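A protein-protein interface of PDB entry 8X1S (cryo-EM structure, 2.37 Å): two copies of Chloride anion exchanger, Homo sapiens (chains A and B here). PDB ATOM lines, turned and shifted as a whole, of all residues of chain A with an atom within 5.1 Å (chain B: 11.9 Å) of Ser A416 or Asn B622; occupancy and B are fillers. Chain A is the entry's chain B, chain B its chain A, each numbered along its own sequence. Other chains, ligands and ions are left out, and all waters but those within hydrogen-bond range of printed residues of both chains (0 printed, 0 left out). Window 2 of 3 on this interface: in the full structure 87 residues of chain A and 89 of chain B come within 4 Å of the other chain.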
ATOM      1  N   LYS A 375      -6.664  -8.935  -3.807  1.00  0.00           N
ATOM      2  CA  LYS A 375      -7.556  -9.998  -4.255  1.00  0.00           C
ATOM      3  C   LYS A 375      -7.161 -11.352  -3.683  1.00  0.00           C
ATOM      4  O   LYS A 375      -8.029 -12.152  -3.330  1.00  0.00           O
ATOM      5  CB  LYS A 375      -7.577 -10.051  -5.777  1.00  0.00           C
ATOM      6  CG  LYS A 375      -8.461 -11.124  -6.329  1.00  0.00           C
ATOM      7  CD  LYS A 375      -8.500 -11.058  -7.825  1.00  0.00           C
ATOM      8  CE  LYS A 375      -9.434 -12.088  -8.389  1.00  0.00           C
ATOM      9  NZ  LYS A 375      -8.831 -12.783  -9.543  1.00  0.00           N
ATOM     10  N   SER A 411      -0.924  -8.047 -17.323  1.00  0.00           N
ATOM     11  CA  SER A 411      -1.016  -8.607 -15.982  1.00  0.00           C
ATOM     12  C   SER A 411      -2.365  -9.266 -15.791  1.00  0.00           C
ATOM     13  O   SER A 411      -2.457 -10.327 -15.179  1.00  0.00           O
ATOM     14  CB  SER A 411      -0.780  -7.523 -14.936  1.00  0.00           C
ATOM     15  OG  SER A 411       0.473  -6.902 -15.129  1.00  0.00           O
ATOM     16  N   ALA A 412      -3.408  -8.652 -16.328  1.00  0.00           N
ATOM     17  CA  ALA A 412      -4.742  -9.224 -16.248  1.00  0.00           C
ATOM     18  C   ALA A 412      -4.797 -10.542 -16.985  1.00  0.00           C
ATOM     19  O   ALA A 412      -5.417 -11.480 -16.510  1.00  0.00           O
ATOM     20  CB  ALA A 412      -5.761  -8.254 -16.811  1.00  0.00           C
ATOM     21  N   VAL A 413      -4.143 -10.628 -18.134  1.00  0.00           N
ATOM     22  CA  VAL A 413      -4.090 -11.881 -18.873  1.00  0.00           C
ATOM     23  C   VAL A 413      -3.431 -12.977 -18.053  1.00  0.00           C
ATOM     24  O   VAL A 413      -3.950 -14.079 -17.960  1.00  0.00           O
ATOM     25  CB  VAL A 413      -3.335 -11.712 -20.207  1.00  0.00           C
ATOM     26  CG1 VAL A 413      -3.084 -13.060 -20.864  1.00  0.00           C
ATOM     27  CG2 VAL A 413      -4.089 -10.780 -21.139  1.00  0.00           C
ATOM     28  N   GLN A 414      -2.303 -12.672 -17.433  1.00  0.00           N
ATOM     29  CA  GLN A 414      -1.591 -13.663 -16.638  1.00  0.00           C
ATOM     30  C   GLN A 414      -2.458 -14.153 -15.495  1.00  0.00           C
ATOM     31  O   GLN A 414      -2.482 -15.340 -15.201  1.00  0.00           O
ATOM     32  CB  GLN A 414      -0.273 -13.086 -16.113  1.00  0.00           C
ATOM     33  CG  GLN A 414       0.526 -14.021 -15.223  1.00  0.00           C
ATOM     34  CD  GLN A 414       1.926 -13.508 -14.954  1.00  0.00           C
ATOM     35  OE1 GLN A 414       2.529 -12.854 -15.799  1.00  0.00           O
ATOM     36  NE2 GLN A 414       2.454 -13.814 -13.776  1.00  0.00           N
ATOM     37  N   GLU A 415      -3.171 -13.246 -14.848  1.00  0.00           N
ATOM     38  CA  GLU A 415      -4.044 -13.624 -13.751  1.00  0.00           C
ATOM     39  C   GLU A 415      -5.302 -14.322 -14.256  1.00  0.00           C
ATOM     40  O   GLU A 415      -5.723 -15.326 -13.696  1.00  0.00           O
ATOM     41  CB  GLU A 415      -4.384 -12.390 -12.903  1.00  0.00           C
ATOM     42  CG  GLU A 415      -5.311 -12.664 -11.735  1.00  0.00           C
ATOM     43  CD  GLU A 415      -6.767 -12.622 -12.139  1.00  0.00           C
ATOM     44  OE1 GLU A 415      -7.120 -11.788 -12.997  1.00  0.00           O
ATOM     45  OE2 GLU A 415      -7.559 -13.419 -11.601  1.00  0.00           O
ATOM     46  N   SER A 416      -5.890 -13.806 -15.323  1.00  0.00           N
ATOM     47  CA  SER A 416      -7.113 -14.384 -15.864  1.00  0.00           C
ATOM     48  C   SER A 416      -6.892 -15.751 -16.481  1.00  0.00           C
ATOM     49  O   SER A 416      -7.808 -16.566 -16.523  1.00  0.00           O
ATOM     50  CB  SER A 416      -7.712 -13.451 -16.905  1.00  0.00           C
ATOM     51  OG  SER A 416      -8.841 -14.038 -17.522  1.00  0.00           O
ATOM     52  N   THR A 417      -5.684 -16.010 -16.960  1.00  0.00           N
ATOM     53  CA  THR A 417      -5.379 -17.295 -17.577  1.00  0.00           C
ATOM     54  C   THR A 417      -4.986 -18.313 -16.532  1.00  0.00           C
ATOM     55  O   THR A 417      -4.613 -19.433 -16.865  1.00  0.00           O
ATOM     56  CB  THR A 417      -4.265 -17.163 -18.623  1.00  0.00           C
ATOM     57  OG1 THR A 417      -3.169 -16.433 -18.061  1.00  0.00           O
ATOM     58  CG2 THR A 417      -4.779 -16.426 -19.844  1.00  0.00           C
ATOM     59  N   GLY A 418      -5.054 -17.931 -15.266  1.00  0.00           N
ATOM     60  CA  GLY A 418      -4.777 -18.878 -14.205  1.00  0.00           C
ATOM     61  C   GLY A 418      -3.440 -18.761 -13.533  1.00  0.00           C
ATOM     62  O   GLY A 418      -2.990 -19.696 -12.885  1.00  0.00           O
ATOM     63  N   ARG B 587     -19.488 -22.532   2.435  1.00  0.00           N
ATOM     64  CA  ARG B 587     -19.482 -23.366   1.238  1.00  0.00           C
ATOM     65  C   ARG B 587     -19.314 -24.841   1.572  1.00  0.00           C
ATOM     66  O   ARG B 587     -20.039 -25.682   1.052  1.00  0.00           O
ATOM     67  CB  ARG B 587     -18.369 -22.933   0.293  1.00  0.00           C
ATOM     68  CG  ARG B 587     -18.643 -21.628  -0.430  1.00  0.00           C
ATOM     69  CD  ARG B 587     -17.501 -21.275  -1.363  1.00  0.00           C
ATOM     70  NE  ARG B 587     -17.983 -20.599  -2.560  1.00  0.00           N
ATOM     71  CZ  ARG B 587     -18.308 -21.220  -3.688  1.00  0.00           C
ATOM     72  NH1 ARG B 587     -18.197 -22.537  -3.780  1.00  0.00           N
ATOM     73  NH2 ARG B 587     -18.743 -20.524  -4.728  1.00  0.00           N
ATOM     74  N   GLU B 617     -12.038 -26.522  -1.666  1.00  0.00           N
ATOM     75  CA  GLU B 617     -12.567 -26.242  -2.995  1.00  0.00           C
ATOM     76  C   GLU B 617     -11.478 -25.804  -3.968  1.00  0.00           C
ATOM     77  O   GLU B 617     -11.547 -26.123  -5.154  1.00  0.00           O
ATOM     78  CB  GLU B 617     -13.663 -25.176  -2.930  1.00  0.00           C
ATOM     79  CG  GLU B 617     -14.956 -25.655  -2.295  1.00  0.00           C
ATOM     80  CD  GLU B 617     -16.079 -24.648  -2.438  1.00  0.00           C
ATOM     81  OE1 GLU B 617     -15.802 -23.507  -2.861  1.00  0.00           O
ATOM     82  OE2 GLU B 617     -17.237 -25.000  -2.129  1.00  0.00           O
ATOM     83  N   GLU B 618     -10.481 -25.073  -3.479  1.00  0.00           N
ATOM     84  CA  GLU B 618      -9.429 -24.569  -4.358  1.00  0.00           C
ATOM     85  C   GLU B 618     -10.034 -23.768  -5.496  1.00  0.00           C
ATOM     86  O   GLU B 618      -9.893 -24.138  -6.658  1.00  0.00           O
ATOM     87  CB  GLU B 618      -8.590 -25.721  -4.907  1.00  0.00           C
ATOM     88  CG  GLU B 618      -7.764 -26.452  -3.861  1.00  0.00           C
ATOM     89  CD  GLU B 618      -6.484 -25.720  -3.505  1.00  0.00           C
ATOM     90  OE1 GLU B 618      -6.184 -24.694  -4.152  1.00  0.00           O
ATOM     91  OE2 GLU B 618      -5.773 -26.173  -2.584  1.00  0.00           O
ATOM     92  N   LEU B 619     -10.712 -22.675  -5.170  1.00  0.00           N
ATOM     93  CA  LEU B 619     -11.368 -21.863  -6.187  1.00  0.00           C
ATOM     94  C   LEU B 619     -10.363 -21.249  -7.145  1.00  0.00           C
ATOM     95  O   LEU B 619      -9.236 -20.953  -6.759  1.00  0.00           O
ATOM     96  CB  LEU B 619     -12.207 -20.762  -5.532  1.00  0.00           C
ATOM     97  CG  LEU B 619     -13.400 -21.159  -4.660  1.00  0.00           C
ATOM     98  CD1 LEU B 619     -12.936 -21.717  -3.325  1.00  0.00           C
ATOM     99  CD2 LEU B 619     -14.289 -19.948  -4.434  1.00  0.00           C
ATOM    100  N   ASP B 620     -10.768 -21.059  -8.395  1.00  0.00           N
ATOM    101  CA  ASP B 620      -9.842 -20.536  -9.395  1.00  0.00           C
ATOM    102  C   ASP B 620      -9.721 -19.026  -9.328  1.00  0.00           C
ATOM    103  O   ASP B 620     -10.396 -18.380  -8.533  1.00  0.00           O
ATOM    104  CB  ASP B 620     -10.246 -20.989 -10.807  1.00  0.00           C
ATOM    105  CG  ASP B 620     -11.543 -20.366 -11.280  1.00  0.00           C
ATOM    106  OD1 ASP B 620     -12.096 -20.848 -12.289  1.00  0.00           O
ATOM    107  OD2 ASP B 620     -12.014 -19.400 -10.656  1.00  0.00           O
ATOM    108  N   ASN B 621      -8.858 -18.462 -10.162  1.00  0.00           N
ATOM    109  CA  ASN B 621      -8.634 -17.026 -10.141  1.00  0.00           C
ATOM    110  C   ASN B 621      -9.884 -16.270 -10.532  1.00  0.00           C
ATOM    111  O   ASN B 621     -10.050 -15.114 -10.164  1.00  0.00           O
ATOM    112  CB  ASN B 621      -7.485 -16.655 -11.080  1.00  0.00           C
ATOM    113  CG  ASN B 621      -6.143 -17.149 -10.588  1.00  0.00           C
ATOM    114  OD1 ASN B 621      -6.065 -18.004  -9.708  1.00  0.00           O
ATOM    115  ND2 ASN B 621      -5.073 -16.611 -11.160  1.00  0.00           N
ATOM    116  N   ASN B 622     -10.770 -16.917 -11.274  1.00  0.00           N
ATOM    117  CA  ASN B 622     -11.967 -16.236 -11.750  1.00  0.00           C
ATOM    118  C   ASN B 622     -13.208 -16.522 -10.910  1.00  0.00           C
ATOM    119  O   ASN B 622     -14.309 -16.142 -11.291  1.00  0.00           O
ATOM    120  CB  ASN B 622     -12.223 -16.609 -13.209  1.00  0.00           C
ATOM    121  CG  ASN B 622     -11.136 -16.106 -14.139  1.00  0.00           C
ATOM    122  OD1 ASN B 622     -11.019 -16.557 -15.277  1.00  0.00           O
ATOM    123  ND2 ASN B 622     -10.329 -15.168 -13.656  1.00  0.00           N
ATOM    124  N   GLN B 623     -13.038 -17.185  -9.775  1.00  0.00           N
ATOM    125  CA  GLN B 623     -14.163 -17.480  -8.899  1.00  0.00           C
ATOM    126  C   GLN B 623     -13.893 -17.099  -7.455  1.00  0.00           C
ATOM    127  O   GLN B 623     -14.810 -17.083  -6.642  1.00  0.00           O
ATOM    128  CB  GLN B 623     -14.491 -18.968  -8.954  1.00  0.00           C
ATOM    129  CG  GLN B 623     -14.976 -19.456 -10.306  1.00  0.00           C
ATOM    130  CD  GLN B 623     -14.797 -20.950 -10.474  1.00  0.00           C
ATOM    131  OE1 GLN B 623     -15.266 -21.538 -11.447  1.00  0.00           O
ATOM    132  NE2 GLN B 623     -14.109 -21.573  -9.522  1.00  0.00           N
ATOM    133  N   ILE B 624     -12.651 -16.782  -7.124  1.00  0.00           N
ATOM    134  CA  ILE B 624     -12.297 -16.494  -5.738  1.00  0.00           C
ATOM    135  C   ILE B 624     -13.010 -15.262  -5.184  1.00  0.00           C
ATOM    136  O   ILE B 624     -13.055 -15.064  -3.975  1.00  0.00           O
ATOM    137  CB  ILE B 624     -10.767 -16.332  -5.594  1.00  0.00           C
ATOM    138  CG1 ILE B 624     -10.350 -16.412  -4.126  1.00  0.00           C
ATOM    139  CG2 ILE B 624     -10.306 -15.030  -6.235  1.00  0.00           C
ATOM    140  CD1 ILE B 624      -8.859 -16.280  -3.913  1.00  0.00           C
ATOM    141  N   GLU B 625     -13.579 -14.444  -6.057  1.00  0.00           N
ATOM    142  CA  GLU B 625     -14.243 -13.220  -5.617  1.00  0.00           C
ATOM    143  C   GLU B 625     -15.553 -13.486  -4.894  1.00  0.00           C
ATOM    144  O   GLU B 625     -16.099 -12.596  -4.247  1.00  0.00           O
ATOM    145  CB  GLU B 625     -14.507 -12.304  -6.813  1.00  0.00           C
ATOM    146  CG  GLU B 625     -13.320 -12.127  -7.747  1.00  0.00           C
ATOM    147  CD  GLU B 625     -13.128 -13.298  -8.696  1.00  0.00           C
ATOM    148  OE1 GLU B 625     -13.984 -14.208  -8.705  1.00  0.00           O
ATOM    149  OE2 GLU B 625     -12.125 -13.307  -9.437  1.00  0.00           O
ATOM    150  N   VAL B 626     -16.067 -14.702  -5.008  1.00  0.00           N
ATOM    151  CA  VAL B 626     -17.325 -15.051  -4.360  1.00  0.00           C
ATOM    152  C   VAL B 626     -17.177 -15.076  -2.843  1.00  0.00           C
ATOM    153  O   VAL B 626     -18.160 -14.923  -2.121  1.00  0.00           O
ATOM    154  CB  VAL B 626     -17.832 -16.415  -4.857  1.00  0.00           C
ATOM    155  CG1 VAL B 626     -16.939 -17.534  -4.347  1.00  0.00           C
ATOM    156  CG2 VAL B 626     -19.272 -16.638  -4.428  1.00  0.00           C
ATOM    157  N   LEU B 627     -15.957 -15.252  -2.355  1.00  0.00           N
ATOM    158  CA  LEU B 627     -15.722 -15.334  -0.920  1.00  0.00           C
ATOM    159  C   LEU B 627     -15.746 -13.966  -0.264  1.00  0.00           C
ATOM    160  O   LEU B 627     -15.490 -13.846   0.930  1.00  0.00           O
ATOM    161  CB  LEU B 627     -14.385 -16.024  -0.653  1.00  0.00           C
ATOM    162  CG  LEU B 627     -14.231 -17.433  -1.215  1.00  0.00           C
ATOM    163  CD1 LEU B 627     -12.832 -17.953  -0.933  1.00  0.00           C
ATOM    164  CD2 LEU B 627     -15.285 -18.357  -0.627  1.00  0.00           C
ATOM    165  N   ASP B 628     -16.056 -12.937  -1.037  1.00  0.00           N
ATOM    166  CA  ASP B 628     -16.086 -11.585  -0.504  1.00  0.00           C
ATOM    167  C   ASP B 628     -17.495 -11.044  -0.466  1.00  0.00           C
ATOM    168  O   ASP B 628     -17.710  -9.893  -0.102  1.00  0.00           O
ATOM    169  CB  ASP B 628     -15.221 -10.665  -1.360  1.00  0.00           C
ATOM    170  CG  ASP B 628     -13.767 -11.088  -1.389  1.00  0.00           C
ATOM    171  OD1 ASP B 628     -13.467 -12.248  -1.042  1.00  0.00           O
ATOM    172  OD2 ASP B 628     -12.919 -10.256  -1.771  1.00  0.00           O
ATOM    173  N   GLN B 629     -18.461 -11.870  -0.836  1.00  0.00           N
ATOM    174  CA  GLN B 629     -19.842 -11.423  -0.885  1.00  0.00           C
ATOM    175  C   GLN B 629     -20.534 -11.557   0.464  1.00  0.00           C
ATOM    176  O   GLN B 629     -20.191 -12.435   1.249  1.00  0.00           O
ATOM    177  CB  GLN B 629     -20.588 -12.218  -1.954  1.00  0.00           C
ATOM    178  CG  GLN B 629     -19.976 -12.100  -3.338  1.00  0.00           C
ATOM    179  CD  GLN B 629     -20.670 -12.978  -4.359  1.00  0.00           C
ATOM    180  OE1 GLN B 629     -21.585 -13.733  -4.026  1.00  0.00           O
ATOM    181  NE2 GLN B 629     -20.238 -12.886  -5.611  1.00  0.00           N
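ND2 of Asn B621 lies within hydrogen-bond range of O of Glu A415 (2.9 Å). O of Asn B621 sits at hydrogen-bond distance from NZ of Lys A375, 2.7 Å away. O of Ser A416 sits close to OD1 of Asn B622 (3.4 Å). OE2 of Glu B625 is in salt-bridge range of NZ of Lys A375.
The side-chain carboxylate (OE2) of Glu A415 is in salt-bridge range of the side-chain amino group (NZ) of Lys A375 (2.5 Å). The side-chain carboxylate (OE1) of Glu B625 lies close to the backbone NH (N) of Gln B623 (3.3 Å). The backbone NH of Asn B622 lies within hydrogen-bond range of the side-chain carboxylate of Asp B620 (2.8 Å).
Among the printed residues, pairs that only touch across the chains: Lys A375 with Ile B624 (3.7 Å), Glu A415 with Asn B622 (3.9 Å) and Gly A418 with Asn B621 (3.6 Å).
Glu A415 touches two residues of chain B. Of chain B, only Asn B622 (3.4 Å) comes within 4 Å of Ser A416. No residue of chain B comes within 4 Å of Thr A417. Asn B622 touches just these residues of chain A: Glu A415 and Ser A416. Printed residues of chain A within 4 Å of Ile B624: Lys A375. Printed residues of chain A within 4 Å of Glu B625: Lys A375 (3.1 Å). Asp B628 touches none of the printed residues of chain A.
Printed residues of chain B that touch a printed residue of chain A: Asn B621, Asn B622, Ile B624 and Glu B625.
No position is printed for both chains. Of the 7 pairs that touch across the chains among the printed residues, none has its exchanged pair printed and touching as well.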
